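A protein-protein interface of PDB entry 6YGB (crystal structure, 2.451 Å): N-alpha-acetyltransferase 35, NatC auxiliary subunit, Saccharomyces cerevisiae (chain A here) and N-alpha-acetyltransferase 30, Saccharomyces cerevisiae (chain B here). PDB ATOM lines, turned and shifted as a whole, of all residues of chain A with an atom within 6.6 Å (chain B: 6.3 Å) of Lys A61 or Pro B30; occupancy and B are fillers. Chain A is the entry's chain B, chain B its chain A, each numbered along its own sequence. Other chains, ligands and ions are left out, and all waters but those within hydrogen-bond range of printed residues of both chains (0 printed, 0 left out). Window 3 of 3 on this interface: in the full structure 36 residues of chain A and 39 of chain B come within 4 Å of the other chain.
Glu A56 touches Ser B32.
O of Ser B28 touches CE of Lys A61, at 3.2 Å.
Pro B30 touches Lys A61.
Pro B30 touches Leu A62 (O to CD1, 3.7 Å).
Leu A62 touches Tyr B31.
N of Ser B32 touches CD1 of Leu A62, 3.9 Å away.
Glu B29 touches Pro A286 (OE2 to CG, 3.5 Å).
Of the 11 printed residues of chain A, 5 touch a printed residue of chain B.
Of the 11 printed residues of chain B, 7 touch a printed residue of chain A.
Hydrophobic or aromatic side chains of chain B that line the printed part of chain A: Pro B30.
Among the printed residues, 10 pairs touch across the chains.
Among the printed residues, Asp or Glu carboxylates within 4 Å of a Lys or Arg side-chain nitrogen of the other chain: Glu A56 with Lys B20 (3.99 Å).
N of Tyr B31 lies within hydrogen-bond range of OD1 of Asp B24.
OD1 of Asn A59 lies within hydrogen-bond range of N of Lys A61 (3.0 Å).
The backbone carbonyl oxygen of Tyr B31 lies within hydrogen-bond range of the side-chain amino group of Lys B20, at 3.2 Å.
The side-chain carboxylate of Asp B24 is in salt-bridge range of the side-chain amino group of Lys B20 (2.8 Å).
The side-chain hydroxyl (OG) of Ser B32 lies within hydrogen-bond range of the backbone NH (N) of Val B35 (3.4 Å).
The backbone NH (N) of Leu A62 lies within hydrogen-bond range of the side-chain amide oxygen (OD1) of Asn A59 (3.4 Å).
Printed residues of chain B within 4 Å of Lys A61: Leu B27, Ser B28 and Pro B30.
Pro B30 touches just these residues of chain A: Lys A61 and Leu A62.
Printed residues of chain A within 4 Å of Glu B29: Pro A286.
Of the printed residues of chain B, Leu A62 touches Pro B30, Tyr B31 and Ser B32.
Of the printed residues of chain A, Leu B27 touches Lys A61 (3.2 Å).
Of the printed residues of chain A, Ser B28 touches Lys A61.
The nearest residue of chain A that does not touch Pro B30 is Asn A59 (4.6 Å).
The nearest printed residue of chain A that does not touch Glu B29 is Leu A62 (4.4 Å).
OG of Ser B32 sits at hydrogen-bond distance from OG of Ser A54, at 2.9 Å.
The side-chain amino group of Lys A61 sits at hydrogen-bond distance from the backbone carbonyl oxygen of Leu B27 (3.2 Å).
OE1 of Glu A56 lies within salt-bridge range of NZ of Lys B20 (3.99 Å).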
ATOM      1  N   SER A  54      -5.585  22.245 -28.586  1.00  0.00           N
ATOM      2  CA  SER A  54      -5.396  23.478 -29.332  1.00  0.00           C
ATOM      3  C   SER A  54      -4.069  24.147 -28.986  1.00  0.00           C
ATOM      4  O   SER A  54      -3.537  23.998 -27.883  1.00  0.00           O
ATOM      5  CB  SER A  54      -6.551  24.448 -29.061  1.00  0.00           C
ATOM      6  OG  SER A  54      -6.654  24.735 -27.681  1.00  0.00           O
ATOM      7  N   GLU A  56      -1.793  27.834 -28.749  1.00  0.00           N
ATOM      8  CA  GLU A  56      -2.061  29.155 -28.196  1.00  0.00           C
ATOM      9  C   GLU A  56      -1.002  30.124 -28.697  1.00  0.00           C
ATOM     10  O   GLU A  56       0.195  29.870 -28.543  1.00  0.00           O
ATOM     11  CB  GLU A  56      -2.085  29.123 -26.667  1.00  0.00           C
ATOM     12  CG  GLU A  56      -2.855  30.273 -26.050  1.00  0.00           C
ATOM     13  CD  GLU A  56      -3.142  30.052 -24.586  1.00  0.00           C
ATOM     14  OE1 GLU A  56      -2.185  30.091 -23.782  1.00  0.00           O
ATOM     15  OE2 GLU A  56      -4.318  29.827 -24.237  1.00  0.00           O
ATOM     16  N   ASN A  59       2.551  32.123 -26.793  1.00  0.00           N
ATOM     17  CA  ASN A  59       2.999  31.255 -25.709  1.00  0.00           C
ATOM     18  C   ASN A  59       4.197  30.482 -26.228  1.00  0.00           C
ATOM     19  O   ASN A  59       4.059  29.690 -27.166  1.00  0.00           O
ATOM     20  CB  ASN A  59       1.891  30.295 -25.252  1.00  0.00           C
ATOM     21  CG  ASN A  59       2.312  29.431 -24.073  1.00  0.00           C
ATOM     22  OD1 ASN A  59       3.409  28.870 -24.056  1.00  0.00           O
ATOM     23  ND2 ASN A  59       1.443  29.327 -23.078  1.00  0.00           N
ATOM     24  N   SER A  60       5.367  30.713 -25.620  1.00  0.00           N
ATOM     25  CA  SER A  60       6.614  30.151 -26.136  1.00  0.00           C
ATOM     26  C   SER A  60       6.516  28.643 -26.334  1.00  0.00           C
ATOM     27  O   SER A  60       6.948  28.114 -27.365  1.00  0.00           O
ATOM     28  CB  SER A  60       7.767  30.488 -25.190  1.00  0.00           C
ATOM     29  OG  SER A  60       7.663  31.821 -24.719  1.00  0.00           O
ATOM     30  N   LYS A  61       5.933  27.940 -25.369  1.00  0.00           N
ATOM     31  CA  LYS A  61       5.886  26.486 -25.397  1.00  0.00           C
ATOM     32  C   LYS A  61       4.735  25.941 -26.236  1.00  0.00           C
ATOM     33  O   LYS A  61       4.699  24.733 -26.497  1.00  0.00           O
ATOM     34  CB  LYS A  61       5.816  25.961 -23.959  1.00  0.00           C
ATOM     35  CG  LYS A  61       6.936  26.519 -23.073  1.00  0.00           C
ATOM     36  CD  LYS A  61       6.587  26.485 -21.587  1.00  0.00           C
ATOM     37  CE  LYS A  61       6.936  25.150 -20.948  1.00  0.00           C
ATOM     38  NZ  LYS A  61       6.553  25.111 -19.508  1.00  0.00           N
ATOM     39  N   LEU A  62       3.817  26.794 -26.688  1.00  0.00           N
ATOM     40  CA  LEU A  62       2.699  26.358 -27.511  1.00  0.00           C
ATOM     41  C   LEU A  62       2.604  27.075 -28.853  1.00  0.00           C
ATOM     42  O   LEU A  62       1.724  26.733 -29.653  1.00  0.00           O
ATOM     43  CB  LEU A  62       1.376  26.537 -26.754  1.00  0.00           C
ATOM     44  CG  LEU A  62       1.103  25.533 -25.633  1.00  0.00           C
ATOM     45  CD1 LEU A  62      -0.080  25.971 -24.781  1.00  0.00           C
ATOM     46  CD2 LEU A  62       0.858  24.145 -26.204  1.00  0.00           C
ATOM     47  N   ASP A  63       3.470  28.048 -29.131  1.00  0.00           N
ATOM     48  CA  ASP A  63       3.439  28.804 -30.380  1.00  0.00           C
ATOM     49  C   ASP A  63       4.678  28.467 -31.204  1.00  0.00           C
ATOM     50  O   ASP A  63       5.803  28.733 -30.773  1.00  0.00           O
ATOM     51  CB  ASP A  63       3.370  30.308 -30.103  1.00  0.00           C
ATOM     52  CG  ASP A  63       2.943  31.121 -31.325  1.00  0.00           C
ATOM     53  OD1 ASP A  63       3.166  30.666 -32.465  1.00  0.00           O
ATOM     54  OD2 ASP A  63       2.393  32.225 -31.143  1.00  0.00           O
ATOM     55  N   SER A  64       4.469  27.907 -32.400  1.00  0.00           N
ATOM     56  CA  SER A  64       5.578  27.517 -33.269  1.00  0.00           C
ATOM     57  C   SER A  64       6.273  28.727 -33.889  1.00  0.00           C
ATOM     58  O   SER A  64       7.462  28.653 -34.233  1.00  0.00           O
ATOM     59  CB  SER A  64       5.066  26.571 -34.365  1.00  0.00           C
ATOM     60  OG  SER A  64       4.268  25.534 -33.809  1.00  0.00           O
ATOM     61  N   LEU A  66       7.146  31.509 -32.509  1.00  0.00           N
ATOM     62  CA  LEU A  66       8.067  32.204 -31.619  1.00  0.00           C
ATOM     63  C   LEU A  66       9.403  31.492 -31.463  1.00  0.00           C
ATOM     64  O   LEU A  66      10.220  31.925 -30.643  1.00  0.00           O
ATOM     65  CB  LEU A  66       7.431  32.393 -30.237  1.00  0.00           C
ATOM     66  CG  LEU A  66       6.054  33.052 -30.220  1.00  0.00           C
ATOM     67  CD1 LEU A  66       5.614  33.333 -28.791  1.00  0.00           C
ATOM     68  CD2 LEU A  66       6.050  34.325 -31.056  1.00  0.00           C
ATOM     69  N   PRO A 286       2.795  21.773 -31.145  1.00  0.00           N
ATOM     70  CA  PRO A 286       3.653  22.735 -30.438  1.00  0.00           C
ATOM     71  C   PRO A 286       5.101  22.583 -30.861  1.00  0.00           C
ATOM     72  O   PRO A 286       5.492  21.528 -31.385  1.00  0.00           O
ATOM     73  CB  PRO A 286       3.463  22.359 -28.959  1.00  0.00           C
ATOM     74  CG  PRO A 286       2.197  21.568 -28.912  1.00  0.00           C
ATOM     75  CD  PRO A 286       2.133  20.840 -30.214  1.00  0.00           C
ATOM     76  N   PRO A 287       5.925  23.614 -30.672  1.00  0.00           N
ATOM     77  CA  PRO A 287       7.352  23.469 -30.974  1.00  0.00           C
ATOM     78  C   PRO A 287       7.980  22.430 -30.064  1.00  0.00           C
ATOM     79  O   PRO A 287       7.629  22.316 -28.889  1.00  0.00           O
ATOM     80  CB  PRO A 287       7.920  24.866 -30.703  1.00  0.00           C
ATOM     81  CG  PRO A 287       6.956  25.483 -29.748  1.00  0.00           C
ATOM     82  CD  PRO A 287       5.610  24.952 -30.140  1.00  0.00           C
ATOM     83  N   LYS B  20      -4.319  28.883 -13.537  1.00  0.00           N
ATOM     84  CA  LYS B  20      -3.563  28.586 -14.748  1.00  0.00           C
ATOM     85  C   LYS B  20      -2.076  28.836 -14.546  1.00  0.00           C
ATOM     86  O   LYS B  20      -1.241  28.042 -14.987  1.00  0.00           O
ATOM     87  CB  LYS B  20      -4.091  29.425 -15.912  1.00  0.00           C
ATOM     88  CG  LYS B  20      -3.221  29.392 -17.154  1.00  0.00           C
ATOM     89  CD  LYS B  20      -3.887  30.127 -18.302  1.00  0.00           C
ATOM     90  CE  LYS B  20      -2.924  30.330 -19.462  1.00  0.00           C
ATOM     91  NZ  LYS B  20      -2.295  29.064 -19.930  1.00  0.00           N
ATOM     92  N   ASP B  24       0.569  25.653 -14.803  1.00  0.00           N
ATOM     93  CA  ASP B  24       1.452  25.666 -15.967  1.00  0.00           C
ATOM     94  C   ASP B  24       2.923  25.554 -15.584  1.00  0.00           C
ATOM     95  O   ASP B  24       3.735  25.099 -16.398  1.00  0.00           O
ATOM     96  CB  ASP B  24       1.227  26.935 -16.789  1.00  0.00           C
ATOM     97  CG  ASP B  24       0.002  26.846 -17.681  1.00  0.00           C
ATOM     98  OD1 ASP B  24      -0.432  25.718 -17.996  1.00  0.00           O
ATOM     99  OD2 ASP B  24      -0.518  27.909 -18.083  1.00  0.00           O
ATOM    100  N   ALA B  25       3.290  25.959 -14.368  1.00  0.00           N
ATOM    101  CA  ALA B  25       4.702  25.973 -13.998  1.00  0.00           C
ATOM    102  C   ALA B  25       5.300  24.570 -13.992  1.00  0.00           C
ATOM    103  O   ALA B  25       6.451  24.376 -14.397  1.00  0.00           O
ATOM    104  CB  ALA B  25       4.877  26.637 -12.634  1.00  0.00           C
ATOM    105  N   LEU B  27       4.177  21.822 -15.640  1.00  0.00           N
ATOM    106  CA  LEU B  27       4.010  21.052 -16.864  1.00  0.00           C
ATOM    107  C   LEU B  27       5.147  21.338 -17.837  1.00  0.00           C
ATOM    108  O   LEU B  27       5.538  22.493 -18.033  1.00  0.00           O
ATOM    109  CB  LEU B  27       2.672  21.381 -17.522  1.00  0.00           C
ATOM    110  CG  LEU B  27       1.434  21.354 -16.626  1.00  0.00           C
ATOM    111  CD1 LEU B  27       0.217  21.807 -17.410  1.00  0.00           C
ATOM    112  CD2 LEU B  27       1.222  19.966 -16.045  1.00  0.00           C
ATOM    113  N   SER B  28       5.675  20.277 -18.450  1.00  0.00           N
ATOM    114  CA  SER B  28       6.667  20.458 -19.503  1.00  0.00           C
ATOM    115  C   SER B  28       6.039  21.099 -20.732  1.00  0.00           C
ATOM    116  O   SER B  28       6.657  21.947 -21.387  1.00  0.00           O
ATOM    117  CB  SER B  28       7.310  19.114 -19.855  1.00  0.00           C
ATOM    118  OG  SER B  28       7.974  18.550 -18.733  1.00  0.00           O
ATOM    119  N   GLU B  29       4.808  20.718 -21.048  1.00  0.00           N
ATOM    120  CA  GLU B  29       4.055  21.285 -22.164  1.00  0.00           C
ATOM    121  C   GLU B  29       2.750  21.851 -21.627  1.00  0.00           C
ATOM    122  O   GLU B  29       1.852  21.075 -21.245  1.00  0.00           O
ATOM    123  CB  GLU B  29       3.784  20.229 -23.233  1.00  0.00           C
ATOM    124  CG  GLU B  29       2.900  20.701 -24.370  1.00  0.00           C
ATOM    125  CD  GLU B  29       2.711  19.634 -25.424  1.00  0.00           C
ATOM    126  OE1 GLU B  29       3.615  18.785 -25.574  1.00  0.00           O
ATOM    127  OE2 GLU B  29       1.658  19.636 -26.095  1.00  0.00           O
ATOM    128  N   PRO B  30       2.599  23.174 -21.577  1.00  0.00           N
ATOM    129  CA  PRO B  30       1.443  23.776 -20.903  1.00  0.00           C
ATOM    130  C   PRO B  30       0.131  23.526 -21.633  1.00  0.00           C
ATOM    131  O   PRO B  30       0.064  22.956 -22.724  1.00  0.00           O
ATOM    132  CB  PRO B  30       1.782  25.271 -20.884  1.00  0.00           C
ATOM    133  CG  PRO B  30       3.258  25.333 -21.049  1.00  0.00           C
ATOM    134  CD  PRO B  30       3.596  24.185 -21.953  1.00  0.00           C
ATOM    135  N   TYR B  31      -0.936  23.979 -20.985  1.00  0.00           N
ATOM    136  CA  TYR B  31      -2.292  23.858 -21.492  1.00  0.00           C
ATOM    137  C   TYR B  31      -2.748  25.209 -22.019  1.00  0.00           C
ATOM    138  O   TYR B  31      -2.394  26.250 -21.460  1.00  0.00           O
ATOM    139  CB  TYR B  31      -3.244  23.389 -20.390  1.00  0.00           C
ATOM    140  CG  TYR B  31      -2.966  22.008 -19.839  1.00  0.00           C
ATOM    141  CD1 TYR B  31      -2.488  20.991 -20.656  1.00  0.00           C
ATOM    142  CD2 TYR B  31      -3.196  21.717 -18.500  1.00  0.00           C
ATOM    143  CE1 TYR B  31      -2.239  19.722 -20.148  1.00  0.00           C
ATOM    144  CE2 TYR B  31      -2.953  20.454 -17.984  1.00  0.00           C
ATOM    145  CZ  TYR B  31      -2.474  19.460 -18.811  1.00  0.00           C
ATOM    146  OH  TYR B  31      -2.232  18.204 -18.299  1.00  0.00           O
ATOM    147  N   SER B  32      -3.530  25.193 -23.096  1.00  0.00           N
ATOM    148  CA  SER B  32      -4.103  26.434 -23.587  1.00  0.00           C
ATOM    149  C   SER B  32      -5.261  26.859 -22.690  1.00  0.00           C
ATOM    150  O   SER B  32      -5.735  26.099 -21.842  1.00  0.00           O
ATOM    151  CB  SER B  32      -4.579  26.284 -25.033  1.00  0.00           C
ATOM    152  OG  SER B  32      -5.834  25.625 -25.100  1.00  0.00           O
ATOM    153  N   VAL B  35      -8.137  24.540 -22.775  1.00  0.00           N
ATOM    154  CA  VAL B  35      -8.022  23.357 -21.928  1.00  0.00           C
ATOM    155  C   VAL B  35      -8.619  23.651 -20.561  1.00  0.00           C
ATOM    156  O   VAL B  35      -9.377  22.850 -20.003  1.00  0.00           O
ATOM    157  CB  VAL B  35      -6.554  22.911 -21.807  1.00  0.00           C
ATOM    158  CG1 VAL B  35      -6.445  21.727 -20.860  1.00  0.00           C
ATOM    159  CG2 VAL B  35      -5.976  22.570 -23.166  1.00  0.00           C
ATOM    160  N   TYR B  36      -8.287  24.818 -20.009  1.00  0.00           N
ATOM    161  CA  TYR B  36      -8.820  25.221 -18.713  1.00  0.00           C
ATOM    162  C   TYR B  36     -10.310  25.535 -18.803  1.00  0.00           C
ATOM    163  O   TYR B  36     -11.066  25.243 -17.869  1.00  0.00           O
ATOM    164  CB  TYR B  36      -8.040  26.427 -18.183  1.00  0.00           C
ATOM    165  CG  TYR B  36      -6.611  26.112 -17.784  1.00  0.00           C
ATOM    166  CD1 TYR B  36      -6.326  25.535 -16.553  1.00  0.00           C
ATOM    167  CD2 TYR B  36      -5.548  26.399 -18.633  1.00  0.00           C
ATOM    168  CE1 TYR B  36      -5.028  25.249 -16.179  1.00  0.00           C
ATOM    169  CE2 TYR B  36      -4.245  26.113 -18.268  1.00  0.00           C
ATOM    170  CZ  TYR B  36      -3.992  25.536 -17.039  1.00  0.00           C
ATOM    171  OH  TYR B  36      -2.701  25.245 -16.663  1.00  0.00           O
